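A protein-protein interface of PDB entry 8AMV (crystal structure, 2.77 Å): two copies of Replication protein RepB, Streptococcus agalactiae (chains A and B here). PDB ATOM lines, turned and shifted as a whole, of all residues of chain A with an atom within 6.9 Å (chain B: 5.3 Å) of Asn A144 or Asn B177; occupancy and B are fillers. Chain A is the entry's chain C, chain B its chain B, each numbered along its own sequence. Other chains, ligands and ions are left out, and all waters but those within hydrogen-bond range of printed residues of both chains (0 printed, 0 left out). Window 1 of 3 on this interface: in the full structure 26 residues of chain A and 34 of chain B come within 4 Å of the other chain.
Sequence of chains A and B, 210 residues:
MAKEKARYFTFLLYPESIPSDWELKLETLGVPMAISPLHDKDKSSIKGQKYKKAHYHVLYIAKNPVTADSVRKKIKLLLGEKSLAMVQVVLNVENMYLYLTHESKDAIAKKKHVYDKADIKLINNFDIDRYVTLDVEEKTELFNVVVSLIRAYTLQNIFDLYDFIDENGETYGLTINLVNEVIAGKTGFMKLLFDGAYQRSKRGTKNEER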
ATOM      1  N   LYS A 139     -16.602  25.965 -19.734  1.00  0.00           N
ATOM      2  CA  LYS A 139     -15.714  27.072 -19.415  1.00  0.00           C
ATOM      3  C   LYS A 139     -15.934  27.532 -17.973  1.00  0.00           C
ATOM      4  O   LYS A 139     -14.974  27.828 -17.252  1.00  0.00           O
ATOM      5  CB  LYS A 139     -15.947  28.205 -20.409  1.00  0.00           C
ATOM      6  CG  LYS A 139     -15.118  29.451 -20.152  1.00  0.00           C
ATOM      7  CD  LYS A 139     -15.975  30.697 -20.067  1.00  0.00           C
ATOM      8  CE  LYS A 139     -15.148  31.869 -19.598  1.00  0.00           C
ATOM      9  NZ  LYS A 139     -15.084  31.878 -18.110  1.00  0.00           N
ATOM     10  N   THR A 140     -17.185  27.485 -17.490  1.00  0.00           N
ATOM     11  CA  THR A 140     -17.457  27.878 -16.107  1.00  0.00           C
ATOM     12  C   THR A 140     -16.828  26.893 -15.127  1.00  0.00           C
ATOM     13  O   THR A 140     -16.296  27.289 -14.083  1.00  0.00           O
ATOM     14  CB  THR A 140     -18.961  27.967 -15.878  1.00  0.00           C
ATOM     15  OG1 THR A 140     -19.431  29.217 -16.365  1.00  0.00           O
ATOM     16  CG2 THR A 140     -19.295  27.867 -14.415  1.00  0.00           C
ATOM     17  N   GLU A 141     -16.862  25.603 -15.450  1.00  0.00           N
ATOM     18  CA  GLU A 141     -16.272  24.640 -14.537  1.00  0.00           C
ATOM     19  C   GLU A 141     -14.764  24.802 -14.532  1.00  0.00           C
ATOM     20  O   GLU A 141     -14.130  24.784 -13.474  1.00  0.00           O
ATOM     21  CB  GLU A 141     -16.673  23.224 -14.955  1.00  0.00           C
ATOM     22  CG  GLU A 141     -16.987  22.260 -13.823  1.00  0.00           C
ATOM     23  CD  GLU A 141     -18.077  21.247 -14.185  1.00  0.00           C
ATOM     24  OE1 GLU A 141     -18.870  21.503 -15.122  1.00  0.00           O
ATOM     25  OE2 GLU A 141     -18.123  20.177 -13.540  1.00  0.00           O
ATOM     26  N   LEU A 142     -14.181  25.015 -15.712  1.00  0.00           N
ATOM     27  CA  LEU A 142     -12.745  25.237 -15.814  1.00  0.00           C
ATOM     28  C   LEU A 142     -12.327  26.486 -15.064  1.00  0.00           C
ATOM     29  O   LEU A 142     -11.273  26.509 -14.415  1.00  0.00           O
ATOM     30  CB  LEU A 142     -12.344  25.340 -17.276  1.00  0.00           C
ATOM     31  CG  LEU A 142     -12.008  24.002 -17.914  1.00  0.00           C
ATOM     32  CD1 LEU A 142     -11.831  24.155 -19.407  1.00  0.00           C
ATOM     33  CD2 LEU A 142     -10.746  23.466 -17.263  1.00  0.00           C
ATOM     34  N   PHE A 143     -13.127  27.549 -15.157  1.00  0.00           N
ATOM     35  CA  PHE A 143     -12.791  28.768 -14.436  1.00  0.00           C
ATOM     36  C   PHE A 143     -12.760  28.520 -12.934  1.00  0.00           C
ATOM     37  O   PHE A 143     -11.792  28.880 -12.253  1.00  0.00           O
ATOM     38  CB  PHE A 143     -13.789  29.872 -14.774  1.00  0.00           C
ATOM     39  CG  PHE A 143     -13.451  31.183 -14.136  1.00  0.00           C
ATOM     40  CD1 PHE A 143     -12.518  32.026 -14.709  1.00  0.00           C
ATOM     41  CD2 PHE A 143     -14.030  31.561 -12.930  1.00  0.00           C
ATOM     42  CE1 PHE A 143     -12.190  33.227 -14.106  1.00  0.00           C
ATOM     43  CE2 PHE A 143     -13.701  32.758 -12.337  1.00  0.00           C
ATOM     44  CZ  PHE A 143     -12.779  33.591 -12.928  1.00  0.00           C
ATOM     45  N   ASN A 144     -13.805  27.886 -12.402  1.00  0.00           N
ATOM     46  CA  ASN A 144     -13.867  27.642 -10.965  1.00  0.00           C
ATOM     47  C   ASN A 144     -12.653  26.839 -10.516  1.00  0.00           C
ATOM     48  O   ASN A 144     -12.180  26.980  -9.380  1.00  0.00           O
ATOM     49  CB  ASN A 144     -15.185  26.949 -10.619  1.00  0.00           C
ATOM     50  CG  ASN A 144     -16.417  27.860 -10.850  1.00  0.00           C
ATOM     51  OD1 ASN A 144     -17.566  27.442 -10.663  1.00  0.00           O
ATOM     52  ND2 ASN A 144     -16.176  29.095 -11.235  1.00  0.00           N
ATOM     53  N   VAL A 145     -12.154  25.958 -11.386  1.00  0.00           N
ATOM     54  CA  VAL A 145     -10.932  25.218 -11.073  1.00  0.00           C
ATOM     55  C   VAL A 145      -9.760  26.173 -10.936  1.00  0.00           C
ATOM     56  O   VAL A 145      -8.995  26.107  -9.965  1.00  0.00           O
ATOM     57  CB  VAL A 145     -10.636  24.146 -12.136  1.00  0.00           C
ATOM     58  CG1 VAL A 145      -9.203  23.666 -11.983  1.00  0.00           C
ATOM     59  CG2 VAL A 145     -11.590  22.998 -11.997  1.00  0.00           C
ATOM     60  N   VAL A 146      -9.582  27.059 -11.925  1.00  0.00           N
ATOM     61  CA  VAL A 146      -8.478  28.016 -11.869  1.00  0.00           C
ATOM     62  C   VAL A 146      -8.539  28.799 -10.569  1.00  0.00           C
ATOM     63  O   VAL A 146      -7.511  29.057  -9.931  1.00  0.00           O
ATOM     64  CB  VAL A 146      -8.497  28.956 -13.092  1.00  0.00           C
ATOM     65  CG1 VAL A 146      -7.520  30.099 -12.900  1.00  0.00           C
ATOM     66  CG2 VAL A 146      -8.177  28.200 -14.357  1.00  0.00           C
ATOM     67  N   VAL A 147      -9.748  29.173 -10.144  1.00  0.00           N
ATOM     68  CA  VAL A 147      -9.898  29.886  -8.880  1.00  0.00           C
ATOM     69  C   VAL A 147      -9.270  29.088  -7.746  1.00  0.00           C
ATOM     70  O   VAL A 147      -8.425  29.594  -6.998  1.00  0.00           O
ATOM     71  CB  VAL A 147     -11.379  30.171  -8.586  1.00  0.00           C
ATOM     72  CG1 VAL A 147     -11.522  30.736  -7.184  1.00  0.00           C
ATOM     73  CG2 VAL A 147     -11.947  31.125  -9.607  1.00  0.00           C
ATOM     74  N   SER A 148      -9.690  27.828  -7.594  1.00  0.00           N
ATOM     75  CA  SER A 148      -9.222  27.030  -6.469  1.00  0.00           C
ATOM     76  C   SER A 148      -7.716  26.852  -6.522  1.00  0.00           C
ATOM     77  O   SER A 148      -7.064  26.751  -5.477  1.00  0.00           O
ATOM     78  CB  SER A 148      -9.924  25.684  -6.444  1.00  0.00           C
ATOM     79  OG  SER A 148      -9.515  24.914  -7.548  1.00  0.00           O
ATOM     80  N   LEU A 149      -7.147  26.797  -7.727  1.00  0.00           N
ATOM     81  CA  LEU A 149      -5.692  26.733  -7.837  1.00  0.00           C
ATOM     82  C   LEU A 149      -5.045  28.010  -7.306  1.00  0.00           C
ATOM     83  O   LEU A 149      -4.031  27.954  -6.597  1.00  0.00           O
ATOM     84  CB  LEU A 149      -5.295  26.497  -9.288  1.00  0.00           C
ATOM     85  CG  LEU A 149      -5.637  25.109  -9.832  1.00  0.00           C
ATOM     86  CD1 LEU A 149      -5.356  25.036 -11.310  1.00  0.00           C
ATOM     87  CD2 LEU A 149      -4.852  24.026  -9.095  1.00  0.00           C
ATOM     88  N   VAL A 182     -10.291  30.620 -21.090  1.00  0.00           N
ATOM     89  CA  VAL A 182     -11.174  30.553 -19.927  1.00  0.00           C
ATOM     90  C   VAL A 182     -11.239  31.891 -19.199  1.00  0.00           C
ATOM     91  O   VAL A 182     -12.301  32.293 -18.722  1.00  0.00           O
ATOM     92  CB  VAL A 182     -10.723  29.411 -18.998  1.00  0.00           C
ATOM     93  CG1 VAL A 182     -11.136  29.682 -17.565  1.00  0.00           C
ATOM     94  CG2 VAL A 182     -11.307  28.091 -19.484  1.00  0.00           C
ATOM     95  N   PHE A 189     -12.203  39.838 -12.563  1.00  0.00           N
ATOM     96  CA  PHE A 189     -12.228  38.777 -11.573  1.00  0.00           C
ATOM     97  C   PHE A 189     -10.800  38.312 -11.288  1.00  0.00           C
ATOM     98  O   PHE A 189     -10.409  38.135 -10.123  1.00  0.00           O
ATOM     99  CB  PHE A 189     -13.072  37.631 -12.121  1.00  0.00           C
ATOM    100  CG  PHE A 189     -13.783  36.807 -11.089  1.00  0.00           C
ATOM    101  CD1 PHE A 189     -13.092  36.178 -10.076  1.00  0.00           C
ATOM    102  CD2 PHE A 189     -15.128  36.572 -11.207  1.00  0.00           C
ATOM    103  CE1 PHE A 189     -13.750  35.382  -9.176  1.00  0.00           C
ATOM    104  CE2 PHE A 189     -15.797  35.799 -10.298  1.00  0.00           C
ATOM    105  CZ  PHE A 189     -15.102  35.202  -9.282  1.00  0.00           C
ATOM    106  N   GLU B   4     -24.903  20.507  -4.260  1.00  0.00           N
ATOM    107  CA  GLU B   4     -25.250  21.784  -4.867  1.00  0.00           C
ATOM    108  C   GLU B   4     -26.566  21.656  -5.636  1.00  0.00           C
ATOM    109  O   GLU B   4     -26.707  20.801  -6.501  1.00  0.00           O
ATOM    110  CB  GLU B   4     -24.108  22.294  -5.760  1.00  0.00           C
ATOM    111  CG  GLU B   4     -23.075  23.089  -4.941  1.00  0.00           C
ATOM    112  CD  GLU B   4     -22.290  24.114  -5.748  1.00  0.00           C
ATOM    113  OE1 GLU B   4     -22.881  24.782  -6.625  1.00  0.00           O
ATOM    114  OE2 GLU B   4     -21.077  24.262  -5.488  1.00  0.00           O
ATOM    115  N   THR B 175     -22.293  29.012  -1.666  1.00  0.00           N
ATOM    116  CA  THR B 175     -21.189  28.127  -1.981  1.00  0.00           C
ATOM    117  C   THR B 175     -20.151  28.935  -2.734  1.00  0.00           C
ATOM    118  O   THR B 175     -20.440  30.025  -3.246  1.00  0.00           O
ATOM    119  CB  THR B 175     -21.656  26.937  -2.830  1.00  0.00           C
ATOM    120  OG1 THR B 175     -21.660  27.311  -4.213  1.00  0.00           O
ATOM    121  CG2 THR B 175     -23.063  26.539  -2.447  1.00  0.00           C
ATOM    122  N   ILE B 176     -18.941  28.381  -2.837  1.00  0.00           N
ATOM    123  CA  ILE B 176     -17.909  29.079  -3.587  1.00  0.00           C
ATOM    124  C   ILE B 176     -18.374  29.315  -5.011  1.00  0.00           C
ATOM    125  O   ILE B 176     -18.382  30.447  -5.496  1.00  0.00           O
ATOM    126  CB  ILE B 176     -16.600  28.289  -3.572  1.00  0.00           C
ATOM    127  CG1 ILE B 176     -16.080  28.172  -2.146  1.00  0.00           C
ATOM    128  CG2 ILE B 176     -15.620  28.984  -4.487  1.00  0.00           C
ATOM    129  CD1 ILE B 176     -15.668  29.477  -1.583  1.00  0.00           C
ATOM    130  N   ASN B 177     -18.821  28.257  -5.680  1.00  0.00           N
ATOM    131  CA  ASN B 177     -19.191  28.408  -7.077  1.00  0.00           C
ATOM    132  C   ASN B 177     -20.390  29.319  -7.226  1.00  0.00           C
ATOM    133  O   ASN B 177     -20.532  29.995  -8.251  1.00  0.00           O
ATOM    134  CB  ASN B 177     -19.453  27.045  -7.713  1.00  0.00           C
ATOM    135  CG  ASN B 177     -18.182  26.286  -7.914  1.00  0.00           C
ATOM    136  OD1 ASN B 177     -17.129  26.709  -7.430  1.00  0.00           O
ATOM    137  ND2 ASN B 177     -18.244  25.181  -8.653  1.00  0.00           N
ATOM    138  N   LEU B 178     -21.231  29.401  -6.201  1.00  0.00           N
ATOM    139  CA  LEU B 178     -22.413  30.235  -6.338  1.00  0.00           C
ATOM    140  C   LEU B 178     -22.071  31.719  -6.184  1.00  0.00           C
ATOM    141  O   LEU B 178     -22.605  32.549  -6.928  1.00  0.00           O
ATOM    142  CB  LEU B 178     -23.463  29.797  -5.316  1.00  0.00           C
ATOM    143  CG  LEU B 178     -24.821  30.506  -5.356  1.00  0.00           C
ATOM    144  CD1 LEU B 178     -25.474  30.426  -6.720  1.00  0.00           C
ATOM    145  CD2 LEU B 178     -25.742  29.957  -4.281  1.00  0.00           C
ATOM    146  N   VAL B 179     -21.116  32.074  -5.305  1.00  0.00           N
ATOM    147  CA  VAL B 179     -20.692  33.478  -5.233  1.00  0.00           C
ATOM    148  C   VAL B 179     -19.957  33.870  -6.505  1.00  0.00           C
ATOM    149  O   VAL B 179     -20.058  35.007  -6.974  1.00  0.00           O
ATOM    150  CB  VAL B 179     -19.840  33.769  -3.978  1.00  0.00           C
ATOM    151  CG1 VAL B 179     -20.595  33.403  -2.711  1.00  0.00           C
ATOM    152  CG2 VAL B 179     -18.470  33.126  -4.042  1.00  0.00           C
ATOM    153  N   ASN B 180     -19.185  32.946  -7.068  1.00  0.00           N
ATOM    154  CA  ASN B 180     -18.509  33.247  -8.314  1.00  0.00           C
ATOM    155  C   ASN B 180     -19.511  33.680  -9.378  1.00  0.00           C
ATOM    156  O   ASN B 180     -19.227  34.583 -10.172  1.00  0.00           O
ATOM    157  CB  ASN B 180     -17.684  32.042  -8.765  1.00  0.00           C
ATOM    158  CG  ASN B 180     -16.487  31.793  -7.860  1.00  0.00           C
ATOM    159  OD1 ASN B 180     -16.306  32.503  -6.868  1.00  0.00           O
ATOM    160  ND2 ASN B 180     -15.650  30.784  -8.196  1.00  0.00           N
ATOM    161  N   GLU B 181     -20.675  33.029  -9.444  1.00  0.00           N
ATOM    162  CA  GLU B 181     -21.649  33.461 -10.435  1.00  0.00           C
ATOM    163  C   GLU B 181     -22.282  34.786 -10.011  1.00  0.00           C
ATOM    164  O   GLU B 181     -22.563  35.653 -10.851  1.00  0.00           O
ATOM    165  CB  GLU B 181     -22.714  32.411 -10.696  1.00  0.00           C
ATOM    166  CG  GLU B 181     -23.685  32.821 -11.841  1.00  0.00           C
ATOM    167  CD  GLU B 181     -22.972  33.134 -13.166  1.00  0.00           C
ATOM    168  OE1 GLU B 181     -23.566  33.803 -14.045  1.00  0.00           O
ATOM    169  OE2 GLU B 181     -21.815  32.694 -13.333  1.00  0.00           O
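Of chain B, only Asn B177 (3.0 Å) and Asn B180 (3.5 Å) come within 4 Å of Asn A144.
Of the printed residues of chain B, Val A147 touches Asn B180.
Of the printed residues of chain B, Phe A189 touches Asn B180 (3.6 Å).
Asn B177 touches one residue of chain A.
The nearest printed residue of chain A that does not touch Asn B180 is Phe A143 (5.0 Å).
No position is printed for both chains.
The backbone carbonyl oxygen (O) of Thr A140 lies close to the side-chain amide nitrogen (ND2) of Asn A144 (3.4 Å).
OG1 of Thr B175 lies close to N of Asn B177, 3.3 Å away.
O of Ile B176 sits close to OD1 of Asn B180, 3.2 Å away.
Among the printed residues, merely in contact across the chains: Asn A144 with Asn B180, Val A147 with Asn B180 and Phe A189 with Asn B180.
ND2 of Asn B177 lies close to OD1 of Asn A144, 3.1 Å away.
Hydrophobic or aromatic side chains of chain A within 4 Å of the printed part of chain B: Val A147 and Phe A189.
Of the 8 printed residues of chain B, 2 touch a printed residue of chain A.
Along chain B the printed residues that touch a printed residue of chain A span positions 177 to 180.
Among the printed residues, 4 pairs touch across the chains.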
